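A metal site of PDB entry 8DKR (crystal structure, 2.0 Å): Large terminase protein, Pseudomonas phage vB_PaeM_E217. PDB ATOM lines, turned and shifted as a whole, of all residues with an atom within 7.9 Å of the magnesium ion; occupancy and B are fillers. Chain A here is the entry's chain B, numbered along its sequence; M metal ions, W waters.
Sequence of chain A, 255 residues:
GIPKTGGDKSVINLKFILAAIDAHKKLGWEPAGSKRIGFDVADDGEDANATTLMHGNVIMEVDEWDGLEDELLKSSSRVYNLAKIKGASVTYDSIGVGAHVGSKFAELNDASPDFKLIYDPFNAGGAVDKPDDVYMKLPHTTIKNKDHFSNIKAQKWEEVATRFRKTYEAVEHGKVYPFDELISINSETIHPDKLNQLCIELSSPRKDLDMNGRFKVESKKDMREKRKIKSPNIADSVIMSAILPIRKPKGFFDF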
ATOM      1  N   PHE A  39      -7.240  14.231  -5.942  1.00  0.00           N
ATOM      2  CA  PHE A  39      -7.986  15.335  -6.560  1.00  0.00           C
ATOM      3  C   PHE A  39      -9.473  15.075  -6.354  1.00  0.00           C
ATOM      4  O   PHE A  39     -10.075  14.260  -7.057  1.00  0.00           O
ATOM      5  CB  PHE A  39      -7.627  15.452  -8.043  1.00  0.00           C
ATOM      6  CG  PHE A  39      -8.447  16.463  -8.807  1.00  0.00           C
ATOM      7  CD1 PHE A  39      -8.960  17.598  -8.189  1.00  0.00           C
ATOM      8  CD2 PHE A  39      -8.681  16.280 -10.168  1.00  0.00           C
ATOM      9  CE1 PHE A  39      -9.710  18.524  -8.907  1.00  0.00           C
ATOM     10  CE2 PHE A  39      -9.431  17.206 -10.886  1.00  0.00           C
ATOM     11  CZ  PHE A  39      -9.941  18.323 -10.257  1.00  0.00           C
ATOM     12  N   ASP A  40     -10.060  15.775  -5.383  1.00  0.00           N
ATOM     13  CA  ASP A  40     -11.507  15.727  -5.178  1.00  0.00           C
ATOM     14  C   ASP A  40     -12.162  16.851  -5.958  1.00  0.00           C
ATOM     15  O   ASP A  40     -11.737  18.015  -5.861  1.00  0.00           O
ATOM     16  CB  ASP A  40     -11.855  15.810  -3.695  1.00  0.00           C
ATOM     17  CG  ASP A  40     -13.322  15.566  -3.433  1.00  0.00           C
ATOM     18  OD1 ASP A  40     -13.828  14.495  -3.840  1.00  0.00           O
ATOM     19  OD2 ASP A  40     -13.984  16.436  -2.813  1.00  0.00           O
ATOM     20  N   VAL A  41     -13.221  16.512  -6.688  1.00  0.00           N
ATOM     21  CA  VAL A  41     -13.837  17.390  -7.685  1.00  0.00           C
ATOM     22  C   VAL A  41     -15.160  17.874  -7.134  1.00  0.00           C
ATOM     23  O   VAL A  41     -16.027  17.073  -6.773  1.00  0.00           O
ATOM     24  CB  VAL A  41     -14.030  16.649  -9.022  1.00  0.00           C
ATOM     25  CG1 VAL A  41     -14.689  17.573 -10.050  1.00  0.00           C
ATOM     26  CG2 VAL A  41     -12.705  16.117  -9.537  1.00  0.00           C
ATOM     27  N   ALA A  42     -15.336  19.197  -7.081  1.00  0.00           N
ATOM     28  CA  ALA A  42     -16.550  19.775  -6.524  1.00  0.00           C
ATOM     29  C   ALA A  42     -17.767  19.423  -7.366  1.00  0.00           C
ATOM     30  O   ALA A  42     -17.692  19.380  -8.605  1.00  0.00           O
ATOM     31  CB  ALA A  42     -16.407  21.294  -6.410  1.00  0.00           C
ATOM     32  N   ASP A  43     -18.886  19.180  -6.697  1.00  0.00           N
ATOM     33  CA  ASP A  43     -20.132  18.800  -7.356  1.00  0.00           C
ATOM     34  C   ASP A  43     -21.284  19.774  -7.155  1.00  0.00           C
ATOM     35  O   ASP A  43     -22.168  19.822  -8.015  1.00  0.00           O
ATOM     36  CB  ASP A  43     -20.577  17.398  -6.891  1.00  0.00           C
ATOM     37  CG  ASP A  43     -19.605  16.320  -7.328  1.00  0.00           C
ATOM     38  OD1 ASP A  43     -19.551  16.018  -8.537  1.00  0.00           O
ATOM     39  OD2 ASP A  43     -18.906  15.766  -6.454  1.00  0.00           O
ATOM     40  N   ASP A  44     -21.288  20.550  -6.070  1.00  0.00           N
ATOM     41  CA  ASP A  44     -22.296  21.580  -5.851  1.00  0.00           C
ATOM     42  C   ASP A  44     -21.618  22.818  -5.287  1.00  0.00           C
ATOM     43  O   ASP A  44     -20.395  22.841  -5.079  1.00  0.00           O
ATOM     44  CB  ASP A  44     -23.396  21.129  -4.894  1.00  0.00           C
ATOM     45  CG  ASP A  44     -23.931  19.754  -5.209  1.00  0.00           C
ATOM     46  OD1 ASP A  44     -24.368  19.522  -6.365  1.00  0.00           O
ATOM     47  OD2 ASP A  44     -23.932  18.891  -4.301  1.00  0.00           O
ATOM     48  N   ASP A  47     -19.680  22.253  -2.181  1.00  0.00           N
ATOM     49  CA  ASP A  47     -18.373  21.623  -2.276  1.00  0.00           C
ATOM     50  C   ASP A  47     -17.342  22.595  -2.829  1.00  0.00           C
ATOM     51  O   ASP A  47     -17.660  23.646  -3.382  1.00  0.00           O
ATOM     52  CB  ASP A  47     -18.437  20.396  -3.201  1.00  0.00           C
ATOM     53  CG  ASP A  47     -18.852  19.135  -2.472  1.00  0.00           C
ATOM     54  OD1 ASP A  47     -19.889  19.167  -1.781  1.00  0.00           O
ATOM     55  OD2 ASP A  47     -18.146  18.122  -2.615  1.00  0.00           O
ATOM     56  N   ALA A  48     -16.083  22.216  -2.641  1.00  0.00           N
ATOM     57  CA  ALA A  48     -14.949  22.887  -3.236  1.00  0.00           C
ATOM     58  C   ALA A  48     -14.015  21.827  -3.809  1.00  0.00           C
ATOM     59  O   ALA A  48     -14.006  20.679  -3.349  1.00  0.00           O
ATOM     60  CB  ALA A  48     -14.195  23.760  -2.229  1.00  0.00           C
ATOM     61  N   ASN A  49     -13.237  22.205  -4.805  1.00  0.00           N
ATOM     62  CA  ASN A  49     -12.213  21.313  -5.330  1.00  0.00           C
ATOM     63  C   ASN A  49     -11.030  21.281  -4.377  1.00  0.00           C
ATOM     64  O   ASN A  49     -10.613  22.317  -3.861  1.00  0.00           O
ATOM     65  CB  ASN A  49     -11.769  21.741  -6.721  1.00  0.00           C
ATOM     66  CG  ASN A  49     -12.935  21.862  -7.688  1.00  0.00           C
ATOM     67  OD1 ASN A  49     -13.478  20.857  -8.140  1.00  0.00           O
ATOM     68  ND2 ASN A  49     -13.323  23.091  -7.987  1.00  0.00           N
ATOM     69  N   TYR A  92      -8.239  10.733  -8.890  1.00  0.00           N
ATOM     70  CA  TYR A  92      -9.267  11.759  -8.845  1.00  0.00           C
ATOM     71  C   TYR A  92     -10.651  11.138  -8.676  1.00  0.00           C
ATOM     72  O   TYR A  92     -10.940  10.056  -9.192  1.00  0.00           O
ATOM     73  CB  TYR A  92      -9.248  12.635 -10.113  1.00  0.00           C
ATOM     74  CG  TYR A  92      -9.667  11.904 -11.369  1.00  0.00           C
ATOM     75  CD1 TYR A  92      -8.764  11.123 -12.084  1.00  0.00           C
ATOM     76  CD2 TYR A  92     -10.970  12.007 -11.859  1.00  0.00           C
ATOM     77  CE1 TYR A  92      -9.144  10.461 -13.233  1.00  0.00           C
ATOM     78  CE2 TYR A  92     -11.359  11.345 -13.004  1.00  0.00           C
ATOM     79  CZ  TYR A  92     -10.446  10.577 -13.691  1.00  0.00           C
ATOM     80  OH  TYR A  92     -10.836   9.925 -14.838  1.00  0.00           O
ATOM     81  N   ASP A  93     -11.495  11.861  -7.946  1.00  0.00           N
ATOM     82  CA  ASP A  93     -12.917  11.545  -7.854  1.00  0.00           C
ATOM     83  C   ASP A  93     -13.545  11.499  -9.245  1.00  0.00           C
ATOM     84  O   ASP A  93     -13.569  12.517  -9.955  1.00  0.00           O
ATOM     85  CB  ASP A  93     -13.620  12.575  -6.966  1.00  0.00           C
ATOM     86  CG  ASP A  93     -15.129  12.374  -6.907  1.00  0.00           C
ATOM     87  OD1 ASP A  93     -15.612  11.261  -7.222  1.00  0.00           O
ATOM     88  OD2 ASP A  93     -15.837  13.334  -6.534  1.00  0.00           O
ATOM     89  N   SER A  94     -14.038  10.329  -9.647  1.00  0.00           N
ATOM     90  CA  SER A  94     -14.486  10.100 -11.012  1.00  0.00           C
ATOM     91  C   SER A  94     -15.993   9.973 -11.152  1.00  0.00           C
ATOM     92  O   SER A  94     -16.477   9.604 -12.235  1.00  0.00           O
ATOM     93  CB  SER A  94     -13.811   8.861 -11.594  1.00  0.00           C
ATOM     94  OG  SER A  94     -14.322   7.679 -10.986  1.00  0.00           O
ATOM     95  N   ILE A  95     -16.766  10.271 -10.111  1.00  0.00           N
ATOM     96  CA  ILE A  95     -18.213  10.220 -10.204  1.00  0.00           C
ATOM     97  C   ILE A  95     -18.747  11.649 -10.201  1.00  0.00           C
ATOM     98  O   ILE A  95     -18.086  12.595  -9.776  1.00  0.00           O
ATOM     99  CB  ILE A  95     -18.855   9.395  -9.069  1.00  0.00           C
ATOM    100  CG1 ILE A  95     -18.483   9.993  -7.709  1.00  0.00           C
ATOM    101  CG2 ILE A  95     -18.423   7.947  -9.150  1.00  0.00           C
ATOM    102  CD1 ILE A  95     -19.036   9.214  -6.535  1.00  0.00           C
ATOM    103  N   GLY A  96     -19.985  11.795 -10.686  1.00  0.00           N
ATOM    104  CA  GLY A  96     -20.536  13.121 -10.849  1.00  0.00           C
ATOM    105  C   GLY A  96     -19.736  13.909 -11.868  1.00  0.00           C
ATOM    106  O   GLY A  96     -19.387  13.406 -12.941  1.00  0.00           O
ATOM    107  N   VAL A  97     -19.420  15.160 -11.515  1.00  0.00           N
ATOM    108  CA  VAL A  97     -18.628  16.031 -12.378  1.00  0.00           C
ATOM    109  C   VAL A  97     -17.299  15.381 -12.736  1.00  0.00           C
ATOM    110  O   VAL A  97     -16.796  15.551 -13.848  1.00  0.00           O
ATOM    111  CB  VAL A  97     -18.424  17.394 -11.686  1.00  0.00           C
ATOM    112  CG1 VAL A  97     -17.626  18.342 -12.590  1.00  0.00           C
ATOM    113  CG2 VAL A  97     -19.758  18.005 -11.313  1.00  0.00           C
ATOM    114  N   GLY A  98     -16.707  14.618 -11.804  1.00  0.00           N
ATOM    115  CA  GLY A  98     -15.445  13.952 -12.083  1.00  0.00           C
ATOM    116  C   GLY A  98     -15.491  12.998 -13.251  1.00  0.00           C
ATOM    117  O   GLY A  98     -14.446  12.693 -13.835  1.00  0.00           O
ATOM    118  N   ALA A  99     -16.690  12.531 -13.632  1.00  0.00           N
ATOM    119  CA  ALA A  99     -16.825  11.693 -14.811  1.00  0.00           C
ATOM    120  C   ALA A  99     -16.358  12.393 -16.075  1.00  0.00           C
ATOM    121  O   ALA A  99     -16.053  11.714 -17.063  1.00  0.00           O
ATOM    122  CB  ALA A  99     -18.285  11.245 -14.971  1.00  0.00           C
ATOM    123  N   LYS A 220     -21.438  11.562   2.868  1.00  0.00           N
ATOM    124  CA  LYS A 220     -21.443  13.024   2.837  1.00  0.00           C
ATOM    125  C   LYS A 220     -22.838  13.562   3.068  1.00  0.00           C
ATOM    126  O   LYS A 220     -23.028  14.544   3.786  1.00  0.00           O
ATOM    127  CB  LYS A 220     -20.882  13.520   1.504  1.00  0.00           C
ATOM    128  CG  LYS A 220     -20.304  14.926   1.556  1.00  0.00           C
ATOM    129  CD  LYS A 220     -19.224  15.099   0.512  1.00  0.00           C
ATOM    130  CE  LYS A 220     -19.823  15.154  -0.887  1.00  0.00           C
ATOM    131  NZ  LYS A 220     -18.814  15.486  -1.919  1.00  0.00           N
ATOM    132  N   ASN A 233     -13.834  18.002   1.687  1.00  0.00           N
ATOM    133  CA  ASN A 233     -13.217  17.760   0.388  1.00  0.00           C
ATOM    134  C   ASN A 233     -11.722  17.504   0.523  1.00  0.00           C
ATOM    135  O   ASN A 233     -11.165  16.654  -0.178  1.00  0.00           O
ATOM    136  CB  ASN A 233     -13.479  18.945  -0.539  1.00  0.00           C
ATOM    137  CG  ASN A 233     -14.953  19.293  -0.647  1.00  0.00           C
ATOM    138  OD1 ASN A 233     -15.402  20.304  -0.115  1.00  0.00           O
ATOM    139  ND2 ASN A 233     -15.703  18.444  -1.347  1.00  0.00           N
ATOM    140  N   ASP A 236     -11.113  13.943   1.598  1.00  0.00           N
ATOM    141  CA  ASP A 236     -11.283  13.028   0.471  1.00  0.00           C
ATOM    142  C   ASP A 236     -10.063  13.054  -0.450  1.00  0.00           C
ATOM    143  O   ASP A 236      -9.586  12.010  -0.903  1.00  0.00           O
ATOM    144  CB  ASP A 236     -12.559  13.362  -0.294  1.00  0.00           C
ATOM    145  CG  ASP A 236     -13.808  13.188   0.544  1.00  0.00           C
ATOM    146  OD1 ASP A 236     -13.878  12.212   1.317  1.00  0.00           O
ATOM    147  OD2 ASP A 236     -14.721  14.025   0.436  1.00  0.00           O
ATOM    148  N   MET A 240      -7.569   9.890  -1.336  1.00  0.00           N
ATOM    149  CA  MET A 240      -7.196   9.516  -2.696  1.00  0.00           C
ATOM    150  C   MET A 240      -5.704   9.662  -2.947  1.00  0.00           C
ATOM    151  O   MET A 240      -5.142   8.904  -3.755  1.00  0.00           O
ATOM    152  CB  MET A 240      -7.998  10.327  -3.705  1.00  0.00           C
ATOM    153  CG  MET A 240      -9.413   9.816  -3.919  1.00  0.00           C
ATOM    154  SD  MET A 240     -10.337  10.779  -5.121  1.00  0.00           S
ATOM    155  CE  MET A 240     -10.464  12.348  -4.254  1.00  0.00           C
HETATM  156 MG    MG M   1     -16.810  14.961  -6.657  1.00  0.00          MG
HETATM  157  O   HOH W   1     -16.810  14.675  -8.669  1.00  0.00           O
HETATM  158  O   HOH W   2     -16.816  15.706  -4.279  1.00  0.00           O
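N of Ile 95 lies close to OD1 of Asp 93. The backbone NH (N) of Asp 93 sits at hydrogen-bond distance from the backbone carbonyl oxygen (O) of Phe 39 (2.9 Å). The backbone NH (N) of Asp 93 sits at hydrogen-bond distance from the side-chain sulfur (SD) of Met 240, at 3.2 Å. The side-chain carboxylate (OD1) of Asp 43 is in hydrogen-bond range of the backbone NH (N) of Val 97, 3.1 Å away.
Three residues have an atom within 4 Å of the magnesium ion: Val 41, Asp 43 and Asp 93.
The magnesium ion is bound by the side-chain carboxylate of Asp 93, water W1, the backbone carbonyl oxygen of Val 41, the side-chain carboxylate of Asp 43 and water W2. The magnesium ion has five donor atoms within binding distance.
Water W2 lies within hydrogen-bond range of the side-chain amino group (NZ) of Lys 220 (3.1 Å), the side-chain carboxylate (OD2) of Asp 47 (3.2 Å) and the side-chain carboxylate (OD1) of Asp 40 (3.3 Å). Water W1 lies within hydrogen-bond range of the backbone carbonyl oxygen (O) of Ile 95 (2.7 Å), the side-chain carboxylate (OD1) of Asp 43 (3.1 Å) and the backbone NH (N) of Gly 98 (3.1 Å).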
